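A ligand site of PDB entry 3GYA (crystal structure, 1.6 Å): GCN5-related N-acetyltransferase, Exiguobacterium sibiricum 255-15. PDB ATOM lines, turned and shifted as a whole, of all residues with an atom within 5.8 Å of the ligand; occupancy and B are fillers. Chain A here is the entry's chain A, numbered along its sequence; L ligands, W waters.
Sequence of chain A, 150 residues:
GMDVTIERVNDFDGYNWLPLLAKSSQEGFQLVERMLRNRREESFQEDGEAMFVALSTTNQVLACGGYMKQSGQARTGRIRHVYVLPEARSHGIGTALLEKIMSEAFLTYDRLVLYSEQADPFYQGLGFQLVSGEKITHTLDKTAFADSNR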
ATOM      1  N   GLU A  27       0.871 -17.023  -0.761  1.00  0.00           N
ATOM      2  CA  GLU A  27       1.639 -16.766   0.443  1.00  0.00           C
ATOM      3  C   GLU A  27       0.788 -16.575   1.698  1.00  0.00           C
ATOM      4  O   GLU A  27       1.330 -16.454   2.780  1.00  0.00           O
ATOM      5  CB  GLU A  27       2.491 -15.518   0.241  1.00  0.00           C
ATOM      6  CG  GLU A  27       3.583 -15.706  -0.750  1.00  0.00           C
ATOM      7  CD  GLU A  27       4.564 -14.568  -0.725  1.00  0.00           C
ATOM      8  OE1 GLU A  27       4.119 -13.427  -0.953  1.00  0.00           O
ATOM      9  OE2 GLU A  27       5.763 -14.826  -0.483  1.00  0.00           O
ATOM     10  N   PHE A  29      -1.462 -13.954   2.102  1.00  0.00           N
ATOM     11  CA  PHE A  29      -1.729 -12.542   2.307  1.00  0.00           C
ATOM     12  C   PHE A  29      -3.058 -12.186   1.603  1.00  0.00           C
ATOM     13  O   PHE A  29      -3.284 -12.587   0.461  1.00  0.00           O
ATOM     14  CB  PHE A  29      -0.649 -11.663   1.668  1.00  0.00           C
ATOM     15  CG  PHE A  29       0.702 -11.779   2.297  1.00  0.00           C
ATOM     16  CD1 PHE A  29       0.925 -11.333   3.601  1.00  0.00           C
ATOM     17  CD2 PHE A  29       1.777 -12.271   1.568  1.00  0.00           C
ATOM     18  CE1 PHE A  29       2.194 -11.409   4.184  1.00  0.00           C
ATOM     19  CE2 PHE A  29       3.050 -12.349   2.141  1.00  0.00           C
ATOM     20  CZ  PHE A  29       3.251 -11.925   3.453  1.00  0.00           C
ATOM     21  N   VAL A  82       1.024  -2.799   1.003  1.00  0.00           N
ATOM     22  CA  VAL A  82       2.354  -2.863   0.420  1.00  0.00           C
ATOM     23  C   VAL A  82       2.728  -4.303   0.149  1.00  0.00           C
ATOM     24  O   VAL A  82       2.774  -5.119   1.056  1.00  0.00           O
ATOM     25  CB  VAL A  82       3.411  -2.285   1.342  1.00  0.00           C
ATOM     26  CG1 VAL A  82       4.807  -2.540   0.789  1.00  0.00           C
ATOM     27  CG2 VAL A  82       3.173  -0.768   1.545  1.00  0.00           C
ATOM     28  N   TYR A  83       3.000  -4.615  -1.104  1.00  0.00           N
ATOM     29  CA  TYR A  83       3.357  -5.974  -1.483  1.00  0.00           C
ATOM     30  C   TYR A  83       4.224  -5.938  -2.738  1.00  0.00           C
ATOM     31  O   TYR A  83       3.884  -5.247  -3.696  1.00  0.00           O
ATOM     32  CB  TYR A  83       2.082  -6.769  -1.799  1.00  0.00           C
ATOM     33  CG  TYR A  83       2.348  -8.197  -2.162  1.00  0.00           C
ATOM     34  CD1 TYR A  83       2.564  -9.148  -1.180  1.00  0.00           C
ATOM     35  CD2 TYR A  83       2.390  -8.619  -3.490  1.00  0.00           C
ATOM     36  CE1 TYR A  83       2.835 -10.494  -1.505  1.00  0.00           C
ATOM     37  CE2 TYR A  83       2.689  -9.935  -3.823  1.00  0.00           C
ATOM     38  CZ  TYR A  83       2.878 -10.878  -2.830  1.00  0.00           C
ATOM     39  OH  TYR A  83       3.156 -12.204  -3.136  1.00  0.00           O
ATOM     40  N   VAL A  84       5.325  -6.691  -2.704  1.00  0.00           N
ATOM     41  CA  VAL A  84       6.225  -6.860  -3.883  1.00  0.00           C
ATOM     42  C   VAL A  84       6.190  -8.319  -4.299  1.00  0.00           C
ATOM     43  O   VAL A  84       6.268  -9.195  -3.443  1.00  0.00           O
ATOM     44  CB  VAL A  84       7.678  -6.472  -3.530  1.00  0.00           C
ATOM     45  CG1 VAL A  84       8.620  -6.735  -4.751  1.00  0.00           C
ATOM     46  CG2 VAL A  84       7.727  -5.015  -3.035  1.00  0.00           C
ATOM     47  N   LEU A  85       6.018  -8.589  -5.590  1.00  0.00           N
ATOM     48  CA  LEU A  85       6.064  -9.979  -6.111  1.00  0.00           C
ATOM     49  C   LEU A  85       7.321 -10.686  -5.605  1.00  0.00           C
ATOM     50  O   LEU A  85       8.396 -10.077  -5.597  1.00  0.00           O
ATOM     51  CB  LEU A  85       6.125  -9.987  -7.638  1.00  0.00           C
ATOM     52  CG  LEU A  85       4.831  -9.932  -8.450  1.00  0.00           C
ATOM     53  CD1 LEU A  85       5.235 -10.070  -9.909  1.00  0.00           C
ATOM     54  CD2 LEU A  85       3.812 -10.987  -8.022  1.00  0.00           C
ATOM     55  N   ALA A  88      10.521 -10.347  -7.538  1.00  0.00           N
ATOM     56  CA  ALA A  88      10.975  -8.958  -7.655  1.00  0.00           C
ATOM     57  C   ALA A  88      11.550  -8.393  -6.344  1.00  0.00           C
ATOM     58  O   ALA A  88      12.008  -7.244  -6.302  1.00  0.00           O
ATOM     59  CB  ALA A  88       9.833  -8.075  -8.138  1.00  0.00           C
ATOM     60  N   ARG A  89      11.524  -9.186  -5.282  1.00  0.00           N
ATOM     61  CA  ARG A  89      12.035  -8.710  -3.984  1.00  0.00           C
ATOM     62  C   ARG A  89      13.553  -8.608  -3.969  1.00  0.00           C
ATOM     63  O   ARG A  89      14.216  -9.232  -4.799  1.00  0.00           O
ATOM     64  CB  ARG A  89      11.559  -9.637  -2.874  1.00  0.00           C
ATOM     65  CG  ARG A  89      10.057  -9.523  -2.660  1.00  0.00           C
ATOM     66  CD  ARG A  89       9.550 -10.570  -1.707  1.00  0.00           C
ATOM     67  NE  ARG A  89       8.111 -10.577  -1.812  1.00  0.00           N
ATOM     68  CZ  ARG A  89       7.320 -11.543  -1.392  1.00  0.00           C
ATOM     69  NH1 ARG A  89       7.818 -12.639  -0.843  1.00  0.00           N
ATOM     70  NH2 ARG A  89       6.004 -11.439  -1.565  1.00  0.00           N
ATOM     71  N   SER A  90      14.070  -7.815  -3.026  1.00  0.00           N
ATOM     72  CA  SER A  90      15.515  -7.669  -2.765  1.00  0.00           C
ATOM     73  C   SER A  90      16.246  -6.939  -3.877  1.00  0.00           C
ATOM     74  O   SER A  90      17.464  -7.115  -4.034  1.00  0.00           O
ATOM     75  CB  SER A  90      16.187  -9.025  -2.512  1.00  0.00           C
ATOM     76  OG  SER A  90      15.475  -9.787  -1.570  1.00  0.00           O
ATOM     77  N   HIS A  91      15.511  -6.153  -4.666  1.00  0.00           N
ATOM     78  CA  HIS A  91      16.081  -5.362  -5.770  1.00  0.00           C
ATOM     79  C   HIS A  91      15.809  -3.867  -5.616  1.00  0.00           C
ATOM     80  O   HIS A  91      15.946  -3.115  -6.578  1.00  0.00           O
ATOM     81  CB  HIS A  91      15.550  -5.857  -7.114  1.00  0.00           C
ATOM     82  CG  HIS A  91      15.986  -7.241  -7.472  1.00  0.00           C
ATOM     83  ND1 HIS A  91      17.275  -7.523  -7.884  1.00  0.00           N
ATOM     84  CD2 HIS A  91      15.324  -8.412  -7.471  1.00  0.00           C
ATOM     85  CE1 HIS A  91      17.376  -8.817  -8.116  1.00  0.00           C
ATOM     86  NE2 HIS A  91      16.213  -9.383  -7.882  1.00  0.00           N
ATOM     87  N   GLY A  92      15.423  -3.439  -4.416  1.00  0.00           N
ATOM     88  CA  GLY A  92      15.206  -2.032  -4.128  1.00  0.00           C
ATOM     89  C   GLY A  92      13.834  -1.472  -4.449  1.00  0.00           C
ATOM     90  O   GLY A  92      13.583  -0.287  -4.255  1.00  0.00           O
ATOM     91  N   ILE A  93      12.921  -2.310  -4.924  1.00  0.00           N
ATOM     92  CA  ILE A  93      11.589  -1.842  -5.308  1.00  0.00           C
ATOM     93  C   ILE A  93      10.747  -1.339  -4.094  1.00  0.00           C
ATOM     94  O   ILE A  93      10.144  -0.264  -4.114  1.00  0.00           O
ATOM     95  CB  ILE A  93      10.818  -2.914  -6.106  1.00  0.00           C
ATOM     96  CG1 ILE A  93      11.523  -3.242  -7.424  1.00  0.00           C
ATOM     97  CG2 ILE A  93       9.358  -2.441  -6.362  1.00  0.00           C
ATOM     98  CD1 ILE A  93      10.943  -4.411  -8.212  1.00  0.00           C
ATOM     99  N   GLY A  94      10.727  -2.124  -3.032  1.00  0.00           N
ATOM    100  CA  GLY A  94       9.947  -1.757  -1.833  1.00  0.00           C
ATOM    101  C   GLY A  94      10.468  -0.455  -1.265  1.00  0.00           C
ATOM    102  O   GLY A  94       9.695   0.441  -0.874  1.00  0.00           O
ATOM    103  N   THR A  95      11.793  -0.316  -1.269  1.00  0.00           N
ATOM    104  CA  THR A  95      12.403   0.920  -0.764  1.00  0.00           C
ATOM    105  C   THR A  95      11.968   2.124  -1.647  1.00  0.00           C
ATOM    106  O   THR A  95      11.550   3.155  -1.122  1.00  0.00           O
ATOM    107  CB  THR A  95      13.930   0.798  -0.709  1.00  0.00           C
ATOM    108  OG1 THR A  95      14.299  -0.183   0.277  1.00  0.00           O
ATOM    109  CG2 THR A  95      14.567   2.173  -0.365  1.00  0.00           C
ATOM    110  N   ALA A  96      12.010   1.981  -2.969  1.00  0.00           N
ATOM    111  CA  ALA A  96      11.593   3.070  -3.854  1.00  0.00           C
ATOM    112  C   ALA A  96      10.110   3.461  -3.649  1.00  0.00           C
ATOM    113  O   ALA A  96       9.742   4.641  -3.558  1.00  0.00           O
ATOM    114  CB  ALA A  96      11.863   2.730  -5.284  1.00  0.00           C
ATOM    115  N   GLN A 118       5.486  -8.989   9.331  1.00  0.00           N
ATOM    116  CA  GLN A 118       6.470  -9.764   8.577  1.00  0.00           C
ATOM    117  C   GLN A 118       7.732  -8.975   8.200  1.00  0.00           C
ATOM    118  O   GLN A 118       8.766  -9.585   7.912  1.00  0.00           O
ATOM    119  CB  GLN A 118       5.826 -10.328   7.295  1.00  0.00           C
ATOM    120  CG  GLN A 118       4.400 -10.903   7.464  1.00  0.00           C
ATOM    121  CD  GLN A 118       3.312  -9.867   7.172  1.00  0.00           C
ATOM    122  N   ALA A 119       7.663  -7.644   8.209  1.00  0.00           N
ATOM    123  CA  ALA A 119       8.703  -6.848   7.574  1.00  0.00           C
ATOM    124  C   ALA A 119       9.328  -5.770   8.482  1.00  0.00           C
ATOM    125  O   ALA A 119       9.666  -4.668   8.031  1.00  0.00           O
ATOM    126  CB  ALA A 119       8.127  -6.238   6.327  1.00  0.00           C
ATOM    127  N   PRO A 121      12.407  -5.477   9.854  1.00  0.00           N
ATOM    128  CA  PRO A 121      13.702  -4.975   9.366  1.00  0.00           C
ATOM    129  C   PRO A 121      13.584  -3.940   8.237  1.00  0.00           C
ATOM    130  O   PRO A 121      14.227  -2.883   8.285  1.00  0.00           O
ATOM    131  CB  PRO A 121      14.364  -6.245   8.822  1.00  0.00           C
ATOM    132  CG  PRO A 121      13.784  -7.331   9.641  1.00  0.00           C
ATOM    133  CD  PRO A 121      12.363  -6.948   9.847  1.00  0.00           C
ATOM    134  N   PHE A 122      12.753  -4.260   7.251  1.00  0.00           N
ATOM    135  CA  PHE A 122      12.453  -3.303   6.196  1.00  0.00           C
ATOM    136  C   PHE A 122      11.995  -1.965   6.772  1.00  0.00           C
ATOM    137  O   PHE A 122      12.567  -0.923   6.444  1.00  0.00           O
ATOM    138  CB  PHE A 122      11.391  -3.866   5.280  1.00  0.00           C
ATOM    139  CG  PHE A 122      10.917  -2.913   4.211  1.00  0.00           C
ATOM    140  CD1 PHE A 122      11.821  -2.389   3.275  1.00  0.00           C
ATOM    141  CD2 PHE A 122       9.580  -2.580   4.089  1.00  0.00           C
ATOM    142  CE1 PHE A 122      11.356  -1.523   2.270  1.00  0.00           C
ATOM    143  CE2 PHE A 122       9.123  -1.745   3.072  1.00  0.00           C
ATOM    144  CZ  PHE A 122       9.998  -1.225   2.160  1.00  0.00           C
ATOM    145  N   TYR A 123      10.968  -1.972   7.623  1.00  0.00           N
ATOM    146  CA  TYR A 123      10.404  -0.697   8.090  1.00  0.00           C
ATOM    147  C   TYR A 123      11.332   0.056   9.029  1.00  0.00           C
ATOM    148  O   TYR A 123      11.411   1.300   8.988  1.00  0.00           O
ATOM    149  CB  TYR A 123       8.992  -0.885   8.656  1.00  0.00           C
ATOM    150  CG  TYR A 123       8.009  -1.143   7.519  1.00  0.00           C
ATOM    151  CD1 TYR A 123       7.784  -0.161   6.549  1.00  0.00           C
ATOM    152  CD2 TYR A 123       7.342  -2.367   7.391  1.00  0.00           C
ATOM    153  CE1 TYR A 123       6.919  -0.374   5.496  1.00  0.00           C
ATOM    154  CE2 TYR A 123       6.458  -2.591   6.334  1.00  0.00           C
ATOM    155  CZ  TYR A 123       6.252  -1.587   5.387  1.00  0.00           C
ATOM    156  OH  TYR A 123       5.395  -1.781   4.322  1.00  0.00           O
HETATM  157  N1  LIG L   1      11.541 -10.439   2.032  1.00  0.00           N
HETATM  158  C1  LIG L   1      11.340  -9.603   3.101  1.00  0.00           C
HETATM  159  N2  LIG L   1      12.146  -8.504   3.303  1.00  0.00           N
HETATM  160  C2  LIG L   1      13.167  -8.251   2.442  1.00  0.00           C
HETATM  161  C3  LIG L   1      13.404  -9.089   1.353  1.00  0.00           C
HETATM  162  C4  LIG L   1      12.575 -10.197   1.156  1.00  0.00           C
HETATM  163  N3  LIG L   1      12.763 -11.078   0.178  1.00  0.00           N
HETATM  164  N4  LIG L   1      14.488  -8.579   0.695  1.00  0.00           N
HETATM  165  C5  LIG L   1      14.905  -7.466   1.333  1.00  0.00           C
HETATM  166  N5  LIG L   1      14.099  -7.251   2.426  1.00  0.00           N
HETATM  167  C6  LIG L   1      14.195  -6.132   3.385  1.00  0.00           C
HETATM  168  C7  LIG L   1      15.613  -5.979   3.926  1.00  0.00           C
HETATM  169  O1  LIG L   1      15.552  -5.532   5.275  1.00  0.00           O
HETATM  170  C8  LIG L   1      16.224  -4.903   3.056  1.00  0.00           C
HETATM  171  O2  LIG L   1      17.321  -4.251   3.663  1.00  0.00           O
HETATM  172  P1  LIG L   1      18.768  -4.233   2.920  1.00  0.00           P
HETATM  173  O3  LIG L   1      19.657  -3.195   3.570  1.00  0.00           O
HETATM  174  O4  LIG L   1      19.381  -5.601   3.058  1.00  0.00           O
HETATM  175  O5  LIG L   1      18.685  -3.892   1.443  1.00  0.00           O
HETATM  176  C9  LIG L   1      15.015  -3.994   2.856  1.00  0.00           C
HETATM  177  O6  LIG L   1      13.889  -4.853   2.798  1.00  0.00           O
HETATM  178  C10 LIG L   1      15.067  -3.110   1.591  1.00  0.00           C
HETATM  179  O7  LIG L   1      15.249  -3.916   0.466  1.00  0.00           O
HETATM  180  P2  LIG L   1      14.320  -3.837  -0.895  1.00  0.00           P
HETATM  181  O8  LIG L   1      13.959  -2.405  -1.156  1.00  0.00           O
HETATM  182  O9  LIG L   1      15.017  -4.629  -1.925  1.00  0.00           O
HETATM  183  O10 LIG L   1      13.019  -4.603  -0.375  1.00  0.00           O
HETATM  184  P3  LIG L   1      11.847  -5.297  -1.226  1.00  0.00           P
HETATM  185  O11 LIG L   1      11.706  -4.727  -2.608  1.00  0.00           O
HETATM  186  O12 LIG L   1      12.063  -6.746  -1.171  1.00  0.00           O
HETATM  187  O13 LIG L   1      10.555  -4.846  -0.378  1.00  0.00           O
HETATM  188  C11 LIG L   1       9.112  -5.910   1.233  1.00  0.00           C
HETATM  189  C12 LIG L   1      10.452  -5.252   0.985  1.00  0.00           C
HETATM  190  C13 LIG L   1       7.989  -4.911   0.925  1.00  0.00           C
HETATM  191  C14 LIG L   1       9.022  -6.345   2.714  1.00  0.00           C
HETATM  192  C15 LIG L   1       8.981  -7.088   0.253  1.00  0.00           C
HETATM  193  O14 LIG L   1      10.078  -7.967   0.311  1.00  0.00           O
HETATM  194  C16 LIG L   1       7.714  -7.879   0.499  1.00  0.00           C
HETATM  195  O15 LIG L   1       6.493  -7.454   0.021  1.00  0.00           O
HETATM  196  N6  LIG L   1       7.788  -9.021   1.162  1.00  0.00           N
HETATM  197  C17 LIG L   1       6.544  -9.741   1.422  1.00  0.00           C
HETATM  198  C18 LIG L   1       6.797 -11.049   2.148  1.00  0.00           C
HETATM  199  C19 LIG L   1       7.369 -10.738   3.501  1.00  0.00           C
HETATM  200  O16 LIG L   1       6.767  -9.941   4.239  1.00  0.00           O
HETATM  201  N7  LIG L   1       8.515 -11.351   3.832  1.00  0.00           N
HETATM  202  C20 LIG L   1       8.707 -12.056   5.088  1.00  0.00           C
HETATM  203  C21 LIG L   1       9.289 -13.460   4.901  1.00  0.00           C
HETATM  204  S1  LIG L   1       8.230 -14.605   3.957  1.00  0.00           S
HETATM  205  O   HOH W   1      17.652  -4.919  -1.495  1.00  0.00           O
HETATM  206  O   HOH W   2      12.917  -5.248  -4.856  1.00  0.00           O
HETATM  207  O   HOH W   3      12.042  -6.949   6.222  1.00  0.00           O
HETATM  208  O   HOH W   4      17.947  -6.858   0.302  1.00  0.00           O
HETATM  209  O   HOH W   5      16.820  -2.417   5.874  1.00  0.00           O
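An oxygen (O12) of the ligand is in hydrogen-bond range of the backbone NH (N) of Ser 90 (2.9 Å). N of Thr 95 sits at hydrogen-bond distance from O8 of the ligand (3.0 Å). The backbone NH of Gly 94 lies within hydrogen-bond range of an oxygen (O11) of the ligand (2.8 Å). OG1 of Thr 95 is in hydrogen-bond range of O8 of the ligand. An oxygen (O15) of the ligand lies within hydrogen-bond range of the backbone NH (N) of Val 84, at 3.1 Å. A nitrogen (N4) of the ligand is in hydrogen-bond range of the side-chain hydroxyl (OG) of Ser 90. The backbone NH (N) of His 91 lies within hydrogen-bond range of an oxygen (O9) of the ligand (3.2 Å). O9 of the ligand is in hydrogen-bond range of N of Gly 92 (2.8 Å).
NH2 of Arg 89 lies close to OH of Tyr 83 (3.3 Å). The side-chain carboxylate (OE1) of Glu 27 is in salt-bridge range of the guanidinium group (NH2) of Arg 89 (2.8 Å). The side-chain hydroxyl (OH) of Tyr 83 sits at hydrogen-bond distance from the side-chain carboxylate (OE1) of Glu 27. The backbone carbonyl oxygen of Val 84 is in hydrogen-bond range of the guanidinium group of Arg 89 (2.8 Å).
The guanidinium group (NE) of Arg 89 sits close to a nitrogen (N6) of the ligand (3.4 Å). Phe 29 touches the ligand (CZ to C18, 3.9 Å). Val 82 touches the ligand. CA of Tyr 83 touches O15 of the ligand, at 3.8 Å. Ile 93 touches the ligand (N to O11, 3.6 Å). Gln 118 touches the ligand (CB to O16, 3.2 Å). Ala 119 touches the ligand (CB to C14, 3.7 Å). Pro 121 touches the ligand. Phe 122 touches the ligand (CD1 to O6, 3.3 Å). Hydrophobic or aromatic side chains within 4 Å of the ligand: Phe 29, Val 82, Val 84, Ala 119, Pro 121 and Phe 122. Of the 20 residues printed, 15 come within 4 Å of the ligand. The nearest printed residue that does not touch the ligand is Ala 88 (4.5 Å).
Water W1 lies within hydrogen-bond range of O9 of the ligand (2.7 Å) and O of Ser 90 (3.4 Å). Water W3 bridges the backbone NH (N) of Phe 122 (3.0 Å) and a nitrogen (N2) of the ligand (3.3 Å).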
